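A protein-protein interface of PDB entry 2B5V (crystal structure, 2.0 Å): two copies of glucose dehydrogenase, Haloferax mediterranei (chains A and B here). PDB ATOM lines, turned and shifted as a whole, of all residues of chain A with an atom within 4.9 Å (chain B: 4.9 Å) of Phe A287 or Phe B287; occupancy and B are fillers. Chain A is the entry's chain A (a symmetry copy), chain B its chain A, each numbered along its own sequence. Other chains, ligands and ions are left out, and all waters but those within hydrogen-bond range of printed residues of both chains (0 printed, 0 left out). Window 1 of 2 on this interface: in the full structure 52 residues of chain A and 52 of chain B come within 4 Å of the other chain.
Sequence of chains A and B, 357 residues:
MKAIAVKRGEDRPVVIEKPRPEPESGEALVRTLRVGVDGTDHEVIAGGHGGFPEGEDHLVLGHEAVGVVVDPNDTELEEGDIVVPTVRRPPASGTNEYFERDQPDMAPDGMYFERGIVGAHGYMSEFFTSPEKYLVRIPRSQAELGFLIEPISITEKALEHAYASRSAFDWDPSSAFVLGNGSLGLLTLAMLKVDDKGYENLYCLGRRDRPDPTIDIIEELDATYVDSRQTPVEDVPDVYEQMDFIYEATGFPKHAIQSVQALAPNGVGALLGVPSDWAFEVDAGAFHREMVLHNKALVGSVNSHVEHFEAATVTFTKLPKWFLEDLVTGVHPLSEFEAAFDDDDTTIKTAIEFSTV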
ATOM      1  N   ALA A 256     -24.445  13.782 -17.366  1.00  0.00           N
ATOM      2  CA  ALA A 256     -24.606  13.690 -15.929  1.00  0.00           C
ATOM      3  C   ALA A 256     -24.804  12.225 -15.515  1.00  0.00           C
ATOM      4  O   ALA A 256     -24.269  11.777 -14.501  1.00  0.00           O
ATOM      5  CB  ALA A 256     -25.783  14.539 -15.490  1.00  0.00           C
ATOM      6  N   ILE A 257     -25.557  11.477 -16.316  1.00  0.00           N
ATOM      7  CA  ILE A 257     -25.823  10.075 -16.031  1.00  0.00           C
ATOM      8  C   ILE A 257     -24.617   9.209 -16.336  1.00  0.00           C
ATOM      9  O   ILE A 257     -24.192   8.382 -15.522  1.00  0.00           O
ATOM     10  CB  ILE A 257     -27.034   9.557 -16.866  1.00  0.00           C
ATOM     11  CG1 ILE A 257     -28.315  10.219 -16.374  1.00  0.00           C
ATOM     12  CG2 ILE A 257     -27.149   8.037 -16.763  1.00  0.00           C
ATOM     13  CD1 ILE A 257     -28.648   9.868 -14.961  1.00  0.00           C
ATOM     14  N   VAL A 260     -21.126   8.618 -14.172  1.00  0.00           N
ATOM     15  CA  VAL A 260     -21.028   7.606 -13.131  1.00  0.00           C
ATOM     16  C   VAL A 260     -20.268   6.373 -13.582  1.00  0.00           C
ATOM     17  O   VAL A 260     -19.536   5.781 -12.798  1.00  0.00           O
ATOM     18  CB  VAL A 260     -22.443   7.247 -12.608  1.00  0.00           C
ATOM     19  CG1 VAL A 260     -22.417   5.998 -11.716  1.00  0.00           C
ATOM     20  CG2 VAL A 260     -22.958   8.433 -11.793  1.00  0.00           C
ATOM     21  N   GLN A 261     -20.421   6.002 -14.849  1.00  0.00           N
ATOM     22  CA  GLN A 261     -19.720   4.840 -15.380  1.00  0.00           C
ATOM     23  C   GLN A 261     -18.252   5.177 -15.645  1.00  0.00           C
ATOM     24  O   GLN A 261     -17.414   4.302 -15.662  1.00  0.00           O
ATOM     25  CB  GLN A 261     -20.367   4.370 -16.685  1.00  0.00           C
ATOM     26  CG  GLN A 261     -21.845   4.004 -16.518  1.00  0.00           C
ATOM     27  CD  GLN A 261     -22.070   3.084 -15.341  1.00  0.00           C
ATOM     28  OE1 GLN A 261     -23.056   3.216 -14.610  1.00  0.00           O
ATOM     29  NE2 GLN A 261     -21.157   2.140 -15.147  1.00  0.00           N
ATOM     30  N   ASP A 283     -30.051   3.239 -18.243  1.00  0.00           N
ATOM     31  CA  ASP A 283     -30.003   2.025 -17.441  1.00  0.00           C
ATOM     32  C   ASP A 283     -29.776   2.538 -15.998  1.00  0.00           C
ATOM     33  O   ASP A 283     -28.639   2.736 -15.553  1.00  0.00           O
ATOM     34  CB  ASP A 283     -28.865   1.094 -17.870  1.00  0.00           C
ATOM     35  CG  ASP A 283     -28.918  -0.246 -17.141  1.00  0.00           C
ATOM     36  OD1 ASP A 283     -29.038  -0.235 -15.893  1.00  0.00           O
ATOM     37  OD2 ASP A 283     -28.856  -1.307 -17.808  1.00  0.00           O
ATOM     38  N   ALA A 284     -30.875   2.812 -15.302  1.00  0.00           N
ATOM     39  CA  ALA A 284     -30.816   3.314 -13.927  1.00  0.00           C
ATOM     40  C   ALA A 284     -30.281   2.288 -12.919  1.00  0.00           C
ATOM     41  O   ALA A 284     -29.718   2.655 -11.885  1.00  0.00           O
ATOM     42  CB  ALA A 284     -32.197   3.801 -13.494  1.00  0.00           C
ATOM     43  N   GLY A 285     -30.444   1.001 -13.209  1.00  0.00           N
ATOM     44  CA  GLY A 285     -29.939  -0.008 -12.289  1.00  0.00           C
ATOM     45  C   GLY A 285     -28.422   0.020 -12.292  1.00  0.00           C
ATOM     46  O   GLY A 285     -27.766  -0.198 -11.266  1.00  0.00           O
ATOM     47  N   ALA A 286     -27.849   0.291 -13.455  1.00  0.00           N
ATOM     48  CA  ALA A 286     -26.405   0.349 -13.594  1.00  0.00           C
ATOM     49  C   ALA A 286     -25.869   1.608 -12.900  1.00  0.00           C
ATOM     50  O   ALA A 286     -24.816   1.576 -12.272  1.00  0.00           O
ATOM     51  CB  ALA A 286     -26.031   0.363 -15.073  1.00  0.00           C
ATOM     52  N   PHE A 287     -26.585   2.713 -13.063  1.00  0.00           N
ATOM     53  CA  PHE A 287     -26.245   4.000 -12.425  1.00  0.00           C
ATOM     54  C   PHE A 287     -26.275   3.820 -10.895  1.00  0.00           C
ATOM     55  O   PHE A 287     -25.313   4.111 -10.176  1.00  0.00           O
ATOM     56  CB  PHE A 287     -27.303   5.034 -12.812  1.00  0.00           C
ATOM     57  CG  PHE A 287     -27.233   6.333 -12.036  1.00  0.00           C
ATOM     58  CD1 PHE A 287     -26.386   7.370 -12.439  1.00  0.00           C
ATOM     59  CD2 PHE A 287     -28.051   6.538 -10.929  1.00  0.00           C
ATOM     60  CE1 PHE A 287     -26.364   8.608 -11.741  1.00  0.00           C
ATOM     61  CE2 PHE A 287     -28.034   7.761 -10.227  1.00  0.00           C
ATOM     62  CZ  PHE A 287     -27.192   8.797 -10.633  1.00  0.00           C
ATOM     63  N   HIS A 288     -27.410   3.334 -10.421  1.00  0.00           N
ATOM     64  CA  HIS A 288     -27.678   3.114  -8.994  1.00  0.00           C
ATOM     65  C   HIS A 288     -26.637   2.189  -8.346  1.00  0.00           C
ATOM     66  O   HIS A 288     -26.036   2.517  -7.307  1.00  0.00           O
ATOM     67  CB  HIS A 288     -29.103   2.511  -8.878  1.00  0.00           C
ATOM     68  CG  HIS A 288     -29.679   2.496  -7.490  1.00  0.00           C
ATOM     69  ND1 HIS A 288     -28.935   2.764  -6.361  1.00  0.00           N
ATOM     70  CD2 HIS A 288     -30.924   2.182  -7.053  1.00  0.00           C
ATOM     71  CE1 HIS A 288     -29.695   2.617  -5.288  1.00  0.00           C
ATOM     72  NE2 HIS A 288     -30.904   2.262  -5.676  1.00  0.00           N
ATOM     73  N   ARG A 289     -26.426   1.024  -8.950  1.00  0.00           N
ATOM     74  CA  ARG A 289     -25.496   0.054  -8.402  1.00  0.00           C
ATOM     75  C   ARG A 289     -24.042   0.526  -8.353  1.00  0.00           C
ATOM     76  O   ARG A 289     -23.345   0.291  -7.364  1.00  0.00           O
ATOM     77  CB  ARG A 289     -25.571  -1.275  -9.175  1.00  0.00           C
ATOM     78  CG  ARG A 289     -24.436  -2.259  -8.794  1.00  0.00           C
ATOM     79  CD  ARG A 289     -24.588  -3.653  -9.419  1.00  0.00           C
ATOM     80  NE  ARG A 289     -25.667  -3.718 -10.401  1.00  0.00           N
ATOM     81  CZ  ARG A 289     -25.541  -3.449 -11.696  1.00  0.00           C
ATOM     82  NH1 ARG A 289     -24.364  -3.098 -12.210  1.00  0.00           N
ATOM     83  NH2 ARG A 289     -26.611  -3.510 -12.477  1.00  0.00           N
ATOM     84  N   GLU A 290     -23.580   1.189  -9.414  1.00  0.00           N
ATOM     85  CA  GLU A 290     -22.197   1.678  -9.450  1.00  0.00           C
ATOM     86  C   GLU A 290     -22.000   2.760  -8.366  1.00  0.00           C
ATOM     87  O   GLU A 290     -20.961   2.797  -7.690  1.00  0.00           O
ATOM     88  CB  GLU A 290     -21.909   2.226 -10.860  1.00  0.00           C
ATOM     89  CG  GLU A 290     -20.485   2.642 -11.138  1.00  0.00           C
ATOM     90  CD  GLU A 290     -19.462   1.533 -10.925  1.00  0.00           C
ATOM     91  OE1 GLU A 290     -18.312   1.878 -10.653  1.00  0.00           O
ATOM     92  OE2 GLU A 290     -19.785   0.335 -11.028  1.00  0.00           O
ATOM     93  N   MET A 291     -23.003   3.619  -8.198  1.00  0.00           N
ATOM     94  CA  MET A 291     -22.963   4.672  -7.184  1.00  0.00           C
ATOM     95  C   MET A 291     -22.752   4.062  -5.804  1.00  0.00           C
ATOM     96  O   MET A 291     -21.941   4.537  -5.010  1.00  0.00           O
ATOM     97  CB  MET A 291     -24.283   5.461  -7.170  1.00  0.00           C
ATOM     98  CG  MET A 291     -24.431   6.499  -8.289  1.00  0.00           C
ATOM     99  SD  MET A 291     -23.489   7.989  -7.955  1.00  0.00           S
ATOM    100  CE  MET A 291     -24.616   8.808  -6.865  1.00  0.00           C
ATOM    101  N   LEU A 298     -22.124  12.475  -6.623  1.00  0.00           N
ATOM    102  CA  LEU A 298     -22.407  13.447  -7.673  1.00  0.00           C
ATOM    103  C   LEU A 298     -22.872  14.651  -6.889  1.00  0.00           C
ATOM    104  O   LEU A 298     -23.778  14.537  -6.042  1.00  0.00           O
ATOM    105  CB  LEU A 298     -23.567  13.012  -8.569  1.00  0.00           C
ATOM    106  CG  LEU A 298     -23.382  12.016  -9.705  1.00  0.00           C
ATOM    107  CD1 LEU A 298     -24.692  11.924 -10.449  1.00  0.00           C
ATOM    108  CD2 LEU A 298     -22.269  12.481 -10.643  1.00  0.00           C
ATOM    109  N   ALA B 256     -33.584   5.968  -6.903  1.00  0.00           N
ATOM    110  CA  ALA B 256     -32.346   6.723  -6.906  1.00  0.00           C
ATOM    111  C   ALA B 256     -32.495   7.974  -7.782  1.00  0.00           C
ATOM    112  O   ALA B 256     -32.009   9.050  -7.434  1.00  0.00           O
ATOM    113  CB  ALA B 256     -31.214   5.846  -7.404  1.00  0.00           C
ATOM    114  N   ILE B 257     -33.189   7.834  -8.907  1.00  0.00           N
ATOM    115  CA  ILE B 257     -33.397   8.944  -9.824  1.00  0.00           C
ATOM    116  C   ILE B 257     -34.434   9.914  -9.294  1.00  0.00           C
ATOM    117  O   ILE B 257     -34.223  11.131  -9.261  1.00  0.00           O
ATOM    118  CB  ILE B 257     -33.862   8.432 -11.222  1.00  0.00           C
ATOM    119  CG1 ILE B 257     -32.719   7.685 -11.899  1.00  0.00           C
ATOM    120  CG2 ILE B 257     -34.325   9.597 -12.097  1.00  0.00           C
ATOM    121  CD1 ILE B 257     -31.540   8.556 -12.185  1.00  0.00           C
ATOM    122  N   VAL B 260     -34.112  12.848  -6.378  1.00  0.00           N
ATOM    123  CA  VAL B 260     -33.663  14.197  -6.689  1.00  0.00           C
ATOM    124  C   VAL B 260     -34.802  15.197  -6.744  1.00  0.00           C
ATOM    125  O   VAL B 260     -34.638  16.340  -6.334  1.00  0.00           O
ATOM    126  CB  VAL B 260     -32.843  14.190  -8.005  1.00  0.00           C
ATOM    127  CG1 VAL B 260     -32.586  15.613  -8.520  1.00  0.00           C
ATOM    128  CG2 VAL B 260     -31.503  13.511  -7.722  1.00  0.00           C
ATOM    129  N   GLN B 261     -35.961  14.761  -7.226  1.00  0.00           N
ATOM    130  CA  GLN B 261     -37.120  15.642  -7.304  1.00  0.00           C
ATOM    131  C   GLN B 261     -37.749  15.821  -5.922  1.00  0.00           C
ATOM    132  O   GLN B 261     -38.411  16.803  -5.670  1.00  0.00           O
ATOM    133  CB  GLN B 261     -38.169  15.069  -8.259  1.00  0.00           C
ATOM    134  CG  GLN B 261     -37.631  14.858  -9.678  1.00  0.00           C
ATOM    135  CD  GLN B 261     -36.912  16.082 -10.198  1.00  0.00           C
ATOM    136  OE1 GLN B 261     -35.882  15.976 -10.870  1.00  0.00           O
ATOM    137  NE2 GLN B 261     -37.450  17.255  -9.892  1.00  0.00           N
ATOM    138  N   ASP B 283     -36.385  11.345 -17.228  1.00  0.00           N
ATOM    139  CA  ASP B 283     -36.198  12.703 -17.716  1.00  0.00           C
ATOM    140  C   ASP B 283     -34.862  13.151 -17.077  1.00  0.00           C
ATOM    141  O   ASP B 283     -34.825  13.675 -15.957  1.00  0.00           O
ATOM    142  CB  ASP B 283     -37.340  13.632 -17.293  1.00  0.00           C
ATOM    143  CG  ASP B 283     -37.227  15.009 -17.942  1.00  0.00           C
ATOM    144  OD1 ASP B 283     -36.124  15.601 -17.880  1.00  0.00           O
ATOM    145  OD2 ASP B 283     -38.227  15.493 -18.524  1.00  0.00           O
ATOM    146  N   ALA B 284     -33.765  12.876 -17.775  1.00  0.00           N
ATOM    147  CA  ALA B 284     -32.429  13.231 -17.291  1.00  0.00           C
ATOM    148  C   ALA B 284     -32.172  14.743 -17.245  1.00  0.00           C
ATOM    149  O   ALA B 284     -31.362  15.221 -16.448  1.00  0.00           O
ATOM    150  CB  ALA B 284     -31.368  12.547 -18.151  1.00  0.00           C
ATOM    151  N   GLY B 285     -32.860  15.508 -18.088  1.00  0.00           N
ATOM    152  CA  GLY B 285     -32.660  16.950 -18.069  1.00  0.00           C
ATOM    153  C   GLY B 285     -33.207  17.519 -16.773  1.00  0.00           C
ATOM    154  O   GLY B 285     -32.664  18.473 -16.203  1.00  0.00           O
ATOM    155  N   ALA B 286     -34.293  16.932 -16.295  1.00  0.00           N
ATOM    156  CA  ALA B 286     -34.916  17.378 -15.062  1.00  0.00           C
ATOM    157  C   ALA B 286     -34.036  16.991 -13.867  1.00  0.00           C
ATOM    158  O   ALA B 286     -33.902  17.751 -12.915  1.00  0.00           O
ATOM    159  CB  ALA B 286     -36.298  16.745 -14.924  1.00  0.00           C
ATOM    160  N   PHE B 287     -33.480  15.786 -13.919  1.00  0.00           N
ATOM    161  CA  PHE B 287     -32.563  15.272 -12.883  1.00  0.00           C
ATOM    162  C   PHE B 287     -31.329  16.192 -12.808  1.00  0.00           C
ATOM    163  O   PHE B 287     -30.960  16.719 -11.753  1.00  0.00           O
ATOM    164  CB  PHE B 287     -32.100  13.873 -13.288  1.00  0.00           C
ATOM    165  CG  PHE B 287     -30.964  13.315 -12.456  1.00  0.00           C
ATOM    166  CD1 PHE B 287     -31.210  12.647 -11.253  1.00  0.00           C
ATOM    167  CD2 PHE B 287     -29.650  13.415 -12.901  1.00  0.00           C
ATOM    168  CE1 PHE B 287     -30.146  12.077 -10.503  1.00  0.00           C
ATOM    169  CE2 PHE B 287     -28.585  12.856 -12.164  1.00  0.00           C
ATOM    170  CZ  PHE B 287     -28.832  12.186 -10.965  1.00  0.00           C
ATOM    171  N   HIS B 288     -30.703  16.365 -13.960  1.00  0.00           N
ATOM    172  CA  HIS B 288     -29.485  17.169 -14.121  1.00  0.00           C
ATOM    173  C   HIS B 288     -29.679  18.615 -13.640  1.00  0.00           C
ATOM    174  O   HIS B 288     -28.893  19.140 -12.831  1.00  0.00           O
ATOM    175  CB  HIS B 288     -29.101  17.133 -15.624  1.00  0.00           C
ATOM    176  CG  HIS B 288     -27.723  17.640 -15.943  1.00  0.00           C
ATOM    177  ND1 HIS B 288     -26.936  18.313 -15.033  1.00  0.00           N
ATOM    178  CD2 HIS B 288     -27.021  17.620 -17.103  1.00  0.00           C
ATOM    179  CE1 HIS B 288     -25.809  18.686 -15.617  1.00  0.00           C
ATOM    180  NE2 HIS B 288     -25.833  18.283 -16.872  1.00  0.00           N
ATOM    181  N   ARG B 289     -30.721  19.269 -14.144  1.00  0.00           N
ATOM    182  CA  ARG B 289     -30.976  20.654 -13.791  1.00  0.00           C
ATOM    183  C   ARG B 289     -31.282  20.887 -12.311  1.00  0.00           C
ATOM    184  O   ARG B 289     -30.793  21.852 -11.720  1.00  0.00           O
ATOM    185  CB  ARG B 289     -32.120  21.234 -14.643  1.00  0.00           C
ATOM    186  CG  ARG B 289     -32.596  22.623 -14.147  1.00  0.00           C
ATOM    187  CD  ARG B 289     -33.612  23.299 -15.078  1.00  0.00           C
ATOM    188  NE  ARG B 289     -34.073  22.417 -16.148  1.00  0.00           N
ATOM    189  CZ  ARG B 289     -35.109  21.589 -16.065  1.00  0.00           C
ATOM    190  NH1 ARG B 289     -35.837  21.514 -14.952  1.00  0.00           N
ATOM    191  NH2 ARG B 289     -35.402  20.813 -17.100  1.00  0.00           N
ATOM    192  N   GLU B 290     -32.090  20.012 -11.711  1.00  0.00           N
ATOM    193  CA  GLU B 290     -32.435  20.161 -10.293  1.00  0.00           C
ATOM    194  C   GLU B 290     -31.169  19.978  -9.427  1.00  0.00           C
ATOM    195  O   GLU B 290     -30.963  20.706  -8.445  1.00  0.00           O
ATOM    196  CB  GLU B 290     -33.518  19.124  -9.942  1.00  0.00           C
ATOM    197  CG  GLU B 290     -34.111  19.219  -8.557  1.00  0.00           C
ATOM    198  CD  GLU B 290     -34.738  20.572  -8.242  1.00  0.00           C
ATOM    199  OE1 GLU B 290     -34.794  20.898  -7.056  1.00  0.00           O
ATOM    200  OE2 GLU B 290     -35.174  21.303  -9.150  1.00  0.00           O
ATOM    201  N   MET B 291     -30.325  19.021  -9.807  1.00  0.00           N
ATOM    202  CA  MET B 291     -29.072  18.763  -9.098  1.00  0.00           C
ATOM    203  C   MET B 291     -28.221  20.026  -9.063  1.00  0.00           C
ATOM    204  O   MET B 291     -27.661  20.393  -8.031  1.00  0.00           O
ATOM    205  CB  MET B 291     -28.270  17.655  -9.803  1.00  0.00           C
ATOM    206  CG  MET B 291     -28.757  16.227  -9.530  1.00  0.00           C
ATOM    207  SD  MET B 291     -28.238  15.635  -7.918  1.00  0.00           S
ATOM    208  CE  MET B 291     -26.585  15.139  -8.307  1.00  0.00           C
ATOM    209  N   LEU B 298     -25.863  13.448  -4.266  1.00  0.00           N
ATOM    210  CA  LEU B 298     -26.268  12.053  -4.133  1.00  0.00           C
ATOM    211  C   LEU B 298     -24.966  11.363  -3.801  1.00  0.00           C
ATOM    212  O   LEU B 298     -23.964  11.537  -4.519  1.00  0.00           O
ATOM    213  CB  LEU B 298     -26.770  11.466  -5.452  1.00  0.00           C
ATOM    214  CG  LEU B 298     -28.187  11.706  -5.956  1.00  0.00           C
ATOM    215  CD1 LEU B 298     -28.372  10.878  -7.204  1.00  0.00           C
ATOM    216  CD2 LEU B 298     -29.205  11.298  -4.892  1.00  0.00           C
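N of Leu A298 is in hydrogen-bond range of O of Leu B298 (2.9 Å).
Of the printed residues of chain B, Phe A287 touches Phe B287 (3.8 Å). Of the printed residues of chain B, Met A291 touches Leu B298. Printed residues of chain B within 4 Å of Leu A298: Met B291 (3.7 Å) and Leu B298 (2.9 Å). Phe B287 touches just one residue of chain A: Phe A287. Printed residues of chain A within 4 Å of His B288: Ala A256. The nearest printed residue of chain B that does not touch Leu A298 is Phe B287 (4.2 Å).
CB of Ala A256 touches CG of His B288 (3.7 Å). Phe A287 touches Phe B287 (CZ to CZ, 3.8 Å). CG of His A288 touches CB of Ala B256, 3.7 Å away. CE of Met A291 touches O of Leu B298, 3.7 Å away. Met B291 touches Leu A298 (CE to O, 3.7 Å).
Of the 14 printed residues of chain B, 5 touch a printed residue of chain A. Hydrophobic or aromatic side chains of chain B within 4 Å of the printed part of chain A: Ala B256, Phe B287, His B288, Met B291 and Leu B298. Of the 14 printed residues of chain A, 5 touch a printed residue of chain B. Among the printed residues, 6 pairs touch across the chains. Among the printed residues, no Asp or Glu carboxylate lies within 4 Å of a Lys or Arg side-chain nitrogen of the other chain.
Ala A256 touches His B288, and with the chains exchanged His A288 touches Ala B256. Phe A287 touches its own counterpart, Phe B287. Met A291 touches Leu B298, and with the chains exchanged Leu A298 touches Met B291. Leu B298 touches its own counterpart, Leu A298. Positions printed for both chains: 256, 257, 260, 261, 283, 284, 285, 286, 287, 288, 289, 290, 291 and 298.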
